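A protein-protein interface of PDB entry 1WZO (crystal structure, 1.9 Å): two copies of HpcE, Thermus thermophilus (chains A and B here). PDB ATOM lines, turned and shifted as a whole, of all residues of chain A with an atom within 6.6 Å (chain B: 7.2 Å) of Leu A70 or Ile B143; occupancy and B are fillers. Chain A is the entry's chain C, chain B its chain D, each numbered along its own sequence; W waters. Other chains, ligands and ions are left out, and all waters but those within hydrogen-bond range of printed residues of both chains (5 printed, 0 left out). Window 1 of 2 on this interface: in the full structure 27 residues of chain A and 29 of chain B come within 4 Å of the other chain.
NH2 of Arg B144 is in salt-bridge range of OE1 of Glu A67 (3.4 Å). The indole nitrogen (NE1) of Trp A72 sits close to the indole nitrogen (NE1) of Trp B72, at 3.3 Å.
O of Ala A69 is in hydrogen-bond range of N of Ala A50, 2.9 Å away. The backbone NH (N) of Thr B138 lies within hydrogen-bond range of the side-chain hydroxyl (OG1) of Thr B136. The backbone carbonyl oxygen of Arg B144 sits at hydrogen-bond distance from the guanidinium group of Arg B148.
CZ3 of Trp B72 touches CG of Leu A47, 3.98 Å away. Glu A67 touches Thr B136. Phe B139 touches Leu A70. Pro A141 touches Phe B139. Arg B140 touches Pro A141. Phe B139 touches Pro A142 (CE1 to CD, 3.4 Å). CE1 of Phe A198 touches NH1 of Arg B144 (3.2 Å). Ile B143 touches Phe A202 (O to CE1, 3.9 Å). Phe A202 touches Arg B144 (CD2 to CG, 3.5 Å). CB of Met A203 touches O of Gly B147, at 3.9 Å.
Of chain B, only Phe B139 (3.5 Å) and Ile B143 (3.7 Å) come within 4 Å of Leu A70. Of chain A, only Leu A70 and Phe A202 come within 4 Å of Ile B143. Of the printed residues of chain A, Arg B144 touches Glu A67 (3.4 Å), Phe A198 (3.2 Å) and Phe A202 (3.5 Å). Printed residues of chain B within 4 Å of Pro A141: Phe B139 and Arg B140. Printed residues of chain B within 4 Å of Pro A142: Phe B139 (3.4 Å). Of the printed residues of chain A, Thr B138 touches Ala A69. Printed residues of chain A within 4 Å of Trp B72: Leu A47 and Trp A72. Pro A68 touches none of the printed residues of chain B. Phe B151 touches none of the printed residues of chain A.
Of the 18 printed residues of chain A, 10 touch a printed residue of chain B. Printed residues of chain B that touch a printed residue of chain A: Trp B72, Thr B136, Thr B138, Phe B139, Arg B140, Ile B143, Arg B144, Gly B147 and Arg B148.
Trp B72 touches its own counterpart, Trp A72. 3 positions are printed for both chains.
Water W4 bridges the backbone carbonyl oxygen (O) of Leu A70 (2.7 Å) and the backbone NH (N) of Ile B143 (3.0 Å). Water W1 lies within hydrogen-bond range of the side-chain carboxylate (OE1) of Glu A67 (2.7 Å) and the guanidinium group (NH2) of Arg B144 (2.9 Å). Water W5 lies within hydrogen-bond range of O of Tyr B134 (2.7 Å), OE2 of Glu A67 (2.8 Å) and NE of Arg B144 (2.8 Å). Water W3 bridges OG1 of Thr B136 and OE2 of Glu A67. Water W2 lies within hydrogen-bond range of the backbone carbonyl oxygen of Phe A198 (2.8 Å) and the guanidinium group of Arg B144 (3.5 Å).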
ATOM      1  N   LEU A  47      16.313  19.692  -0.593  1.00  0.00           N
ATOM      2  CA  LEU A  47      15.840  19.500   0.780  1.00  0.00           C
ATOM      3  C   LEU A  47      17.005  19.670   1.741  1.00  0.00           C
ATOM      4  O   LEU A  47      18.147  19.366   1.403  1.00  0.00           O
ATOM      5  CB  LEU A  47      15.275  18.095   0.993  1.00  0.00           C
ATOM      6  CG  LEU A  47      14.068  17.620   0.196  1.00  0.00           C
ATOM      7  CD1 LEU A  47      14.488  17.291  -1.231  1.00  0.00           C
ATOM      8  CD2 LEU A  47      13.490  16.391   0.883  1.00  0.00           C
ATOM      9  N   GLY A  48      16.703  20.138   2.944  1.00  0.00           N
ATOM     10  CA  GLY A  48      17.730  20.317   3.951  1.00  0.00           C
ATOM     11  C   GLY A  48      17.227  19.804   5.286  1.00  0.00           C
ATOM     12  O   GLY A  48      16.018  19.755   5.520  1.00  0.00           O
ATOM     13  N   VAL A  49      18.148  19.402   6.157  1.00  0.00           N
ATOM     14  CA  VAL A  49      17.776  18.916   7.477  1.00  0.00           C
ATOM     15  C   VAL A  49      18.248  19.949   8.494  1.00  0.00           C
ATOM     16  O   VAL A  49      19.421  20.323   8.512  1.00  0.00           O
ATOM     17  CB  VAL A  49      18.422  17.543   7.782  1.00  0.00           C
ATOM     18  CG1 VAL A  49      19.935  17.644   7.713  1.00  0.00           C
ATOM     19  CG2 VAL A  49      17.977  17.052   9.164  1.00  0.00           C
ATOM     20  N   ALA A  50      17.324  20.430   9.321  1.00  0.00           N
ATOM     21  CA  ALA A  50      17.654  21.427  10.337  1.00  0.00           C
ATOM     22  C   ALA A  50      18.102  20.756  11.628  1.00  0.00           C
ATOM     23  O   ALA A  50      17.764  19.599  11.881  1.00  0.00           O
ATOM     24  CB  ALA A  50      16.448  22.317  10.607  1.00  0.00           C
ATOM     25  N   GLU A  67      13.329  12.123  14.366  1.00  0.00           N
ATOM     26  CA  GLU A  67      13.197  12.122  12.912  1.00  0.00           C
ATOM     27  C   GLU A  67      13.786  13.403  12.341  1.00  0.00           C
ATOM     28  O   GLU A  67      13.723  14.465  12.966  1.00  0.00           O
ATOM     29  CB  GLU A  67      11.727  11.995  12.492  1.00  0.00           C
ATOM     30  CG  GLU A  67      10.906  13.259  12.673  1.00  0.00           C
ATOM     31  CD  GLU A  67       9.441  13.047  12.337  1.00  0.00           C
ATOM     32  OE1 GLU A  67       8.765  12.305  13.084  1.00  0.00           O
ATOM     33  OE2 GLU A  67       8.967  13.614  11.327  1.00  0.00           O
ATOM     34  N   PRO A  68      14.381  13.320  11.142  1.00  0.00           N
ATOM     35  CA  PRO A  68      14.971  14.509  10.522  1.00  0.00           C
ATOM     36  C   PRO A  68      13.945  15.614  10.266  1.00  0.00           C
ATOM     37  O   PRO A  68      12.885  15.363   9.691  1.00  0.00           O
ATOM     38  CB  PRO A  68      15.557  13.964   9.220  1.00  0.00           C
ATOM     39  CG  PRO A  68      15.885  12.537   9.560  1.00  0.00           C
ATOM     40  CD  PRO A  68      14.682  12.107  10.361  1.00  0.00           C
ATOM     41  N   ALA A  69      14.258  16.832  10.699  1.00  0.00           N
ATOM     42  CA  ALA A  69      13.370  17.974  10.479  1.00  0.00           C
ATOM     43  C   ALA A  69      13.711  18.510   9.089  1.00  0.00           C
ATOM     44  O   ALA A  69      14.619  19.333   8.933  1.00  0.00           O
ATOM     45  CB  ALA A  69      13.612  19.042  11.526  1.00  0.00           C
ATOM     46  N   LEU A  70      12.975  18.037   8.089  1.00  0.00           N
ATOM     47  CA  LEU A  70      13.215  18.421   6.700  1.00  0.00           C
ATOM     48  C   LEU A  70      12.570  19.726   6.262  1.00  0.00           C
ATOM     49  O   LEU A  70      11.415  20.002   6.592  1.00  0.00           O
ATOM     50  CB  LEU A  70      12.737  17.298   5.779  1.00  0.00           C
ATOM     51  CG  LEU A  70      13.234  15.898   6.141  1.00  0.00           C
ATOM     52  CD1 LEU A  70      12.619  14.882   5.200  1.00  0.00           C
ATOM     53  CD2 LEU A  70      14.752  15.852   6.066  1.00  0.00           C
ATOM     54  N   PHE A  71      13.322  20.527   5.511  1.00  0.00           N
ATOM     55  CA  PHE A  71      12.797  21.780   4.992  1.00  0.00           C
ATOM     56  C   PHE A  71      13.193  21.943   3.525  1.00  0.00           C
ATOM     57  O   PHE A  71      14.101  21.268   3.035  1.00  0.00           O
ATOM     58  CB  PHE A  71      13.273  22.982   5.820  1.00  0.00           C
ATOM     59  CG  PHE A  71      14.754  23.216   5.769  1.00  0.00           C
ATOM     60  CD1 PHE A  71      15.623  22.445   6.535  1.00  0.00           C
ATOM     61  CD2 PHE A  71      15.279  24.222   4.960  1.00  0.00           C
ATOM     62  CE1 PHE A  71      17.002  22.674   6.498  1.00  0.00           C
ATOM     63  CE2 PHE A  71      16.653  24.459   4.915  1.00  0.00           C
ATOM     64  CZ  PHE A  71      17.514  23.685   5.685  1.00  0.00           C
ATOM     65  N   TRP A  72      12.506  22.850   2.841  1.00  0.00           N
ATOM     66  CA  TRP A  72      12.716  23.099   1.418  1.00  0.00           C
ATOM     67  C   TRP A  72      13.413  24.413   1.093  1.00  0.00           C
ATOM     68  O   TRP A  72      13.285  25.407   1.814  1.00  0.00           O
ATOM     69  CB  TRP A  72      11.347  23.052   0.721  1.00  0.00           C
ATOM     70  CG  TRP A  72      11.289  23.507  -0.712  1.00  0.00           C
ATOM     71  CD1 TRP A  72      11.904  22.930  -1.789  1.00  0.00           C
ATOM     72  CD2 TRP A  72      10.504  24.590  -1.233  1.00  0.00           C
ATOM     73  NE1 TRP A  72      11.541  23.582  -2.948  1.00  0.00           N
ATOM     74  CE2 TRP A  72      10.684  24.603  -2.635  1.00  0.00           C
ATOM     75  CE3 TRP A  72       9.663  25.547  -0.650  1.00  0.00           C
ATOM     76  CZ2 TRP A  72      10.051  25.537  -3.463  1.00  0.00           C
ATOM     77  CZ3 TRP A  72       9.032  26.476  -1.473  1.00  0.00           C
ATOM     78  CH2 TRP A  72       9.231  26.462  -2.867  1.00  0.00           C
ATOM     79  N   PRO A 141       6.941  25.775   8.404  1.00  0.00           N
ATOM     80  CA  PRO A 141       8.174  25.756   7.607  1.00  0.00           C
ATOM     81  C   PRO A 141       8.786  27.151   7.442  1.00  0.00           C
ATOM     82  O   PRO A 141       8.074  28.136   7.238  1.00  0.00           O
ATOM     83  CB  PRO A 141       7.735  25.129   6.274  1.00  0.00           C
ATOM     84  CG  PRO A 141       6.235  25.236   6.277  1.00  0.00           C
ATOM     85  CD  PRO A 141       5.857  25.053   7.719  1.00  0.00           C
ATOM     86  N   PRO A 142      10.122  27.250   7.549  1.00  0.00           N
ATOM     87  CA  PRO A 142      10.859  28.513   7.422  1.00  0.00           C
ATOM     88  C   PRO A 142      11.085  28.922   5.972  1.00  0.00           C
ATOM     89  O   PRO A 142      12.225  29.046   5.528  1.00  0.00           O
ATOM     90  CB  PRO A 142      12.165  28.208   8.141  1.00  0.00           C
ATOM     91  CG  PRO A 142      12.411  26.789   7.733  1.00  0.00           C
ATOM     92  CD  PRO A 142      11.038  26.145   7.892  1.00  0.00           C
ATOM     93  N   LEU A 195      20.053  10.092   6.060  1.00  0.00           N
ATOM     94  CA  LEU A 195      19.129  11.091   5.553  1.00  0.00           C
ATOM     95  C   LEU A 195      18.531  10.622   4.233  1.00  0.00           C
ATOM     96  O   LEU A 195      17.323  10.733   4.022  1.00  0.00           O
ATOM     97  CB  LEU A 195      19.847  12.432   5.370  1.00  0.00           C
ATOM     98  CG  LEU A 195      20.286  13.104   6.674  1.00  0.00           C
ATOM     99  CD1 LEU A 195      21.156  14.312   6.373  1.00  0.00           C
ATOM    100  CD2 LEU A 195      19.058  13.514   7.478  1.00  0.00           C
ATOM    101  N   PHE A 198      16.016   7.832   4.959  1.00  0.00           N
ATOM    102  CA  PHE A 198      14.779   8.355   5.531  1.00  0.00           C
ATOM    103  C   PHE A 198      13.923   9.049   4.477  1.00  0.00           C
ATOM    104  O   PHE A 198      12.712   8.834   4.405  1.00  0.00           O
ATOM    105  CB  PHE A 198      15.093   9.350   6.643  1.00  0.00           C
ATOM    106  CG  PHE A 198      13.873   9.926   7.299  1.00  0.00           C
ATOM    107  CD1 PHE A 198      13.169   9.198   8.253  1.00  0.00           C
ATOM    108  CD2 PHE A 198      13.421  11.195   6.956  1.00  0.00           C
ATOM    109  CE1 PHE A 198      12.028   9.732   8.860  1.00  0.00           C
ATOM    110  CE2 PHE A 198      12.283  11.737   7.555  1.00  0.00           C
ATOM    111  CZ  PHE A 198      11.586  11.004   8.508  1.00  0.00           C
ATOM    112  N   ILE A 199      14.560   9.885   3.663  1.00  0.00           N
ATOM    113  CA  ILE A 199      13.859  10.624   2.619  1.00  0.00           C
ATOM    114  C   ILE A 199      13.359   9.742   1.482  1.00  0.00           C
ATOM    115  O   ILE A 199      12.182   9.801   1.117  1.00  0.00           O
ATOM    116  CB  ILE A 199      14.764  11.723   2.020  1.00  0.00           C
ATOM    117  CG1 ILE A 199      15.114  12.750   3.098  1.00  0.00           C
ATOM    118  CG2 ILE A 199      14.059  12.403   0.845  1.00  0.00           C
ATOM    119  CD1 ILE A 199      16.148  13.773   2.652  1.00  0.00           C
ATOM    120  N   PHE A 202       9.880   7.550   1.338  1.00  0.00           N
ATOM    121  CA  PHE A 202       8.574   8.072   0.949  1.00  0.00           C
ATOM    122  C   PHE A 202       8.591   8.990  -0.271  1.00  0.00           C
ATOM    123  O   PHE A 202       7.543   9.284  -0.848  1.00  0.00           O
ATOM    124  CB  PHE A 202       7.952   8.823   2.131  1.00  0.00           C
ATOM    125  CG  PHE A 202       8.665  10.104   2.492  1.00  0.00           C
ATOM    126  CD1 PHE A 202       8.425  11.277   1.780  1.00  0.00           C
ATOM    127  CD2 PHE A 202       9.563  10.138   3.555  1.00  0.00           C
ATOM    128  CE1 PHE A 202       9.067  12.470   2.123  1.00  0.00           C
ATOM    129  CE2 PHE A 202      10.210  11.320   3.907  1.00  0.00           C
ATOM    130  CZ  PHE A 202       9.962  12.493   3.190  1.00  0.00           C
ATOM    131  N   MET A 203       9.778   9.439  -0.662  1.00  0.00           N
ATOM    132  CA  MET A 203       9.912  10.356  -1.786  1.00  0.00           C
ATOM    133  C   MET A 203      11.043   9.967  -2.725  1.00  0.00           C
ATOM    134  O   MET A 203      12.193   9.831  -2.301  1.00  0.00           O
ATOM    135  CB  MET A 203      10.157  11.766  -1.248  1.00  0.00           C
ATOM    136  CG  MET A 203      10.467  12.799  -2.299  1.00  0.00           C
ATOM    137  SD  MET A 203      10.794  14.384  -1.529  1.00  0.00           S
ATOM    138  CE  MET A 203      12.511  14.350  -1.432  1.00  0.00           C
ATOM    139  N   LEU A 211      20.613  17.477  -1.342  1.00  0.00           N
ATOM    140  CA  LEU A 211      20.340  17.358   0.086  1.00  0.00           C
ATOM    141  C   LEU A 211      21.327  18.212   0.878  1.00  0.00           C
ATOM    142  O   LEU A 211      22.537  18.036   0.761  1.00  0.00           O
ATOM    143  CB  LEU A 211      20.469  15.897   0.528  1.00  0.00           C
ATOM    144  CG  LEU A 211      20.506  15.628   2.036  1.00  0.00           C
ATOM    145  CD1 LEU A 211      19.190  16.049   2.681  1.00  0.00           C
ATOM    146  CD2 LEU A 211      20.764  14.145   2.273  1.00  0.00           C
ATOM    147  N   TRP B  72       5.659  23.312   1.238  1.00  0.00           N
ATOM    148  CA  TRP B  72       6.045  22.800  -0.072  1.00  0.00           C
ATOM    149  C   TRP B  72       5.490  21.429  -0.427  1.00  0.00           C
ATOM    150  O   TRP B  72       5.275  20.587   0.442  1.00  0.00           O
ATOM    151  CB  TRP B  72       7.579  22.764  -0.133  1.00  0.00           C
ATOM    152  CG  TRP B  72       8.185  22.114  -1.354  1.00  0.00           C
ATOM    153  CD1 TRP B  72       8.041  22.510  -2.655  1.00  0.00           C
ATOM    154  CD2 TRP B  72       9.093  21.002  -1.371  1.00  0.00           C
ATOM    155  NE1 TRP B  72       8.810  21.719  -3.478  1.00  0.00           N
ATOM    156  CE2 TRP B  72       9.465  20.786  -2.719  1.00  0.00           C
ATOM    157  CE3 TRP B  72       9.632  20.170  -0.379  1.00  0.00           C
ATOM    158  CZ2 TRP B  72      10.353  19.771  -3.101  1.00  0.00           C
ATOM    159  CZ3 TRP B  72      10.519  19.158  -0.758  1.00  0.00           C
ATOM    160  CH2 TRP B  72      10.870  18.972  -2.111  1.00  0.00           C
ATOM    161  N   LYS B  73       5.242  21.236  -1.718  1.00  0.00           N
ATOM    162  CA  LYS B  73       4.783  19.963  -2.260  1.00  0.00           C
ATOM    163  C   LYS B  73       5.785  19.656  -3.371  1.00  0.00           C
ATOM    164  O   LYS B  73       5.895  20.409  -4.335  1.00  0.00           O
ATOM    165  CB  LYS B  73       3.368  20.076  -2.852  1.00  0.00           C
ATOM    166  CG  LYS B  73       2.245  20.198  -1.819  1.00  0.00           C
ATOM    167  CD  LYS B  73       1.966  18.881  -1.068  1.00  0.00           C
ATOM    168  CE  LYS B  73       1.342  17.822  -1.973  1.00  0.00           C
ATOM    169  NZ  LYS B  73       0.542  16.808  -1.217  1.00  0.00           N
ATOM    170  N   PRO B  74       6.542  18.557  -3.238  1.00  0.00           N
ATOM    171  CA  PRO B  74       7.540  18.157  -4.234  1.00  0.00           C
ATOM    172  C   PRO B  74       6.922  17.768  -5.570  1.00  0.00           C
ATOM    173  O   PRO B  74       5.791  17.294  -5.619  1.00  0.00           O
ATOM    174  CB  PRO B  74       8.250  16.986  -3.554  1.00  0.00           C
ATOM    175  CG  PRO B  74       7.162  16.381  -2.723  1.00  0.00           C
ATOM    176  CD  PRO B  74       6.513  17.600  -2.117  1.00  0.00           C
ATOM    177  N   TYR B 134       1.807  10.798   9.843  1.00  0.00           N
ATOM    178  CA  TYR B 134       3.115  11.450   9.833  1.00  0.00           C
ATOM    179  C   TYR B 134       3.143  12.934  10.185  1.00  0.00           C
ATOM    180  O   TYR B 134       4.208  13.554  10.148  1.00  0.00           O
ATOM    181  CB  TYR B 134       3.755  11.261   8.457  1.00  0.00           C
ATOM    182  CG  TYR B 134       3.989   9.817   8.099  1.00  0.00           C
ATOM    183  CD1 TYR B 134       5.003   9.089   8.714  1.00  0.00           C
ATOM    184  CD2 TYR B 134       3.178   9.165   7.167  1.00  0.00           C
ATOM    185  CE1 TYR B 134       5.208   7.750   8.413  1.00  0.00           C
ATOM    186  CE2 TYR B 134       3.375   7.823   6.859  1.00  0.00           C
ATOM    187  CZ  TYR B 134       4.393   7.125   7.488  1.00  0.00           C
ATOM    188  OH  TYR B 134       4.603   5.800   7.196  1.00  0.00           O
ATOM    189  N   THR B 136       3.323  16.314  12.310  1.00  0.00           N
ATOM    190  CA  THR B 136       3.985  16.707  13.552  1.00  0.00           C
ATOM    191  C   THR B 136       3.817  18.212  13.747  1.00  0.00           C
ATOM    192  O   THR B 136       3.067  18.861  13.014  1.00  0.00           O
ATOM    193  CB  THR B 136       5.506  16.379  13.533  1.00  0.00           C
ATOM    194  OG1 THR B 136       6.164  17.178  12.540  1.00  0.00           O
ATOM    195  CG2 THR B 136       5.737  14.906  13.220  1.00  0.00           C
ATOM    196  N   THR B 138       6.547  20.261  13.808  1.00  0.00           N
ATOM    197  CA  THR B 138       7.817  20.823  13.359  1.00  0.00           C
ATOM    198  C   THR B 138       7.683  21.038  11.851  1.00  0.00           C
ATOM    199  O   THR B 138       7.573  20.070  11.091  1.00  0.00           O
ATOM    200  CB  THR B 138       8.983  19.853  13.656  1.00  0.00           C
ATOM    201  OG1 THR B 138       9.005  19.550  15.059  1.00  0.00           O
ATOM    202  CG2 THR B 138      10.323  20.482  13.263  1.00  0.00           C
ATOM    203  N   PHE B 139       7.667  22.303  11.429  1.00  0.00           N
ATOM    204  CA  PHE B 139       7.511  22.650  10.011  1.00  0.00           C
ATOM    205  C   PHE B 139       6.240  21.985   9.477  1.00  0.00           C
ATOM    206  O   PHE B 139       6.243  21.347   8.417  1.00  0.00           O
ATOM    207  CB  PHE B 139       8.721  22.177   9.200  1.00  0.00           C
ATOM    208  CG  PHE B 139      10.046  22.665   9.731  1.00  0.00           C
ATOM    209  CD1 PHE B 139      10.156  23.916  10.336  1.00  0.00           C
ATOM    210  CD2 PHE B 139      11.192  21.892   9.582  1.00  0.00           C
ATOM    211  CE1 PHE B 139      11.390  24.391  10.779  1.00  0.00           C
ATOM    212  CE2 PHE B 139      12.435  22.358  10.022  1.00  0.00           C
ATOM    213  CZ  PHE B 139      12.533  23.609  10.619  1.00  0.00           C
ATOM    214  N   ARG B 140       5.154  22.148  10.227  1.00  0.00           N
ATOM    215  CA  ARG B 140       3.863  21.559   9.891  1.00  0.00           C
ATOM    216  C   ARG B 140       3.113  22.262   8.761  1.00  0.00           C
ATOM    217  O   ARG B 140       3.048  23.490   8.719  1.00  0.00           O
ATOM    218  CB  ARG B 140       2.988  21.528  11.146  1.00  0.00           C
ATOM    219  CG  ARG B 140       1.584  21.033  10.912  1.00  0.00           C
ATOM    220  CD  ARG B 140       0.867  20.807  12.228  1.00  0.00           C
ATOM    221  NE  ARG B 140      -0.455  20.224  12.031  1.00  0.00           N
ATOM    222  CZ  ARG B 140      -1.101  19.522  12.957  1.00  0.00           C
ATOM    223  NH1 ARG B 140      -0.539  19.319  14.143  1.00  0.00           N
ATOM    224  NH2 ARG B 140      -2.305  19.025  12.697  1.00  0.00           N
ATOM    225  N   PRO B 141       2.540  21.485   7.822  1.00  0.00           N
ATOM    226  CA  PRO B 141       2.566  20.017   7.773  1.00  0.00           C
ATOM    227  C   PRO B 141       3.907  19.529   7.219  1.00  0.00           C
ATOM    228  O   PRO B 141       4.374  20.011   6.185  1.00  0.00           O
ATOM    229  CB  PRO B 141       1.394  19.688   6.855  1.00  0.00           C
ATOM    230  CG  PRO B 141       1.441  20.810   5.874  1.00  0.00           C
ATOM    231  CD  PRO B 141       1.677  22.024   6.754  1.00  0.00           C
ATOM    232  N   PRO B 142       4.532  18.547   7.892  1.00  0.00           N
ATOM    233  CA  PRO B 142       5.828  18.010   7.463  1.00  0.00           C
ATOM    234  C   PRO B 142       5.862  17.418   6.062  1.00  0.00           C
ATOM    235  O   PRO B 142       4.859  16.912   5.556  1.00  0.00           O
ATOM    236  CB  PRO B 142       6.138  16.973   8.537  1.00  0.00           C
ATOM    237  CG  PRO B 142       4.774  16.447   8.868  1.00  0.00           C
ATOM    238  CD  PRO B 142       3.953  17.716   8.963  1.00  0.00           C
ATOM    239  N   ILE B 143       7.038  17.485   5.446  1.00  0.00           N
ATOM    240  CA  ILE B 143       7.243  16.957   4.107  1.00  0.00           C
ATOM    241  C   ILE B 143       6.896  15.471   4.032  1.00  0.00           C
ATOM    242  O   ILE B 143       6.298  15.026   3.055  1.00  0.00           O
ATOM    243  CB  ILE B 143       8.711  17.158   3.657  1.00  0.00           C
ATOM    244  CG1 ILE B 143       8.995  18.652   3.471  1.00  0.00           C
ATOM    245  CG2 ILE B 143       8.978  16.383   2.369  1.00  0.00           C
ATOM    246  CD1 ILE B 143      10.453  18.970   3.156  1.00  0.00           C
ATOM    247  N   ARG B 144       7.259  14.706   5.058  1.00  0.00           N
ATOM    248  CA  ARG B 144       6.975  13.272   5.049  1.00  0.00           C
ATOM    249  C   ARG B 144       5.478  12.956   5.029  1.00  0.00           C
ATOM    250  O   ARG B 144       5.075  11.867   4.614  1.00  0.00           O
ATOM    251  CB  ARG B 144       7.634  12.571   6.247  1.00  0.00           C
ATOM    252  CG  ARG B 144       7.509  11.049   6.183  1.00  0.00           C
ATOM    253  CD  ARG B 144       8.428  10.319   7.156  1.00  0.00           C
ATOM    254  NE  ARG B 144       8.024  10.494   8.547  1.00  0.00           N
ATOM    255  CZ  ARG B 144       8.361   9.664   9.531  1.00  0.00           C
ATOM    256  NH1 ARG B 144       9.109   8.597   9.274  1.00  0.00           N
ATOM    257  NH2 ARG B 144       7.938   9.893  10.768  1.00  0.00           N
ATOM    258  N   ALA B 145       4.656  13.908   5.459  1.00  0.00           N
ATOM    259  CA  ALA B 145       3.210  13.703   5.480  1.00  0.00           C
ATOM    260  C   ALA B 145       2.520  14.201   4.205  1.00  0.00           C
ATOM    261  O   ALA B 145       1.529  13.622   3.765  1.00  0.00           O
ATOM    262  CB  ALA B 145       2.601  14.402   6.699  1.00  0.00           C
ATOM    263  N   LYS B 146       3.055  15.268   3.618  1.00  0.00           N
ATOM    264  CA  LYS B 146       2.467  15.872   2.425  1.00  0.00           C
ATOM    265  C   LYS B 146       3.193  15.607   1.107  1.00  0.00           C
ATOM    266  O   LYS B 146       2.576  15.660   0.039  1.00  0.00           O
ATOM    267  CB  LYS B 146       2.367  17.389   2.625  1.00  0.00           C
ATOM    268  CG  LYS B 146       1.614  17.823   3.877  1.00  0.00           C
ATOM    269  CD  LYS B 146       0.110  17.674   3.722  1.00  0.00           C
ATOM    270  CE  LYS B 146      -0.457  18.707   2.762  1.00  0.00           C
ATOM    271  NZ  LYS B 146      -1.937  18.582   2.608  1.00  0.00           N
ATOM    272  N   GLY B 147       4.491  15.316   1.172  1.00  0.00           N
ATOM    273  CA  GLY B 147       5.253  15.110  -0.050  1.00  0.00           C
ATOM    274  C   GLY B 147       5.597  13.701  -0.493  1.00  0.00           C
ATOM    275  O   GLY B 147       6.656  13.484  -1.090  1.00  0.00           O
ATOM    276  N   ARG B 148       4.721  12.742  -0.216  1.00  0.00           N
ATOM    277  CA  ARG B 148       4.973  11.367  -0.627  1.00  0.00           C
ATOM    278  C   ARG B 148       4.635  11.252  -2.110  1.00  0.00           C
ATOM    279  O   ARG B 148       3.889  12.078  -2.645  1.00  0.00           O
ATOM    280  CB  ARG B 148       4.110  10.401   0.197  1.00  0.00           C
ATOM    281  CG  ARG B 148       4.211  10.638   1.707  1.00  0.00           C
ATOM    282  CD  ARG B 148       3.388   9.628   2.505  1.00  0.00           C
ATOM    283  NE  ARG B 148       4.046   8.324   2.604  1.00  0.00           N
ATOM    284  CZ  ARG B 148       5.048   8.052   3.437  1.00  0.00           C
ATOM    285  NH1 ARG B 148       5.514   8.993   4.249  1.00  0.00           N
ATOM    286  NH2 ARG B 148       5.579   6.835   3.466  1.00  0.00           N
ATOM    287  N   PHE B 151       1.053  11.980  -4.069  1.00  0.00           N
ATOM    288  CA  PHE B 151       0.172  12.743  -3.190  1.00  0.00           C
ATOM    289  C   PHE B 151      -0.304  14.074  -3.744  1.00  0.00           C
ATOM    290  O   PHE B 151      -0.758  14.941  -2.996  1.00  0.00           O
ATOM    291  CB  PHE B 151       0.828  12.966  -1.824  1.00  0.00           C
ATOM    292  CG  PHE B 151       0.472  11.917  -0.812  1.00  0.00           C
ATOM    293  CD1 PHE B 151       0.439  12.229   0.545  1.00  0.00           C
ATOM    294  CD2 PHE B 151       0.143  10.624  -1.215  1.00  0.00           C
ATOM    295  CE1 PHE B 151       0.079  11.265   1.488  1.00  0.00           C
ATOM    296  CE2 PHE B 151      -0.219   9.655  -0.283  1.00  0.00           C
ATOM    297  CZ  PHE B 151      -0.253   9.975   1.072  1.00  0.00           C
HETATM  298  O   HOH W   1       6.458  10.899  13.080  1.00  0.00           O
HETATM  299  O   HOH W   2      10.638   8.119   6.209  1.00  0.00           O
HETATM  300  O   HOH W   3       8.702  16.404  11.694  1.00  0.00           O
HETATM  301  O   HOH W   4       9.265  18.512   7.165  1.00  0.00           O
HETATM  302  O   HOH W   5       6.740  12.526  10.019  1.00  0.00           O
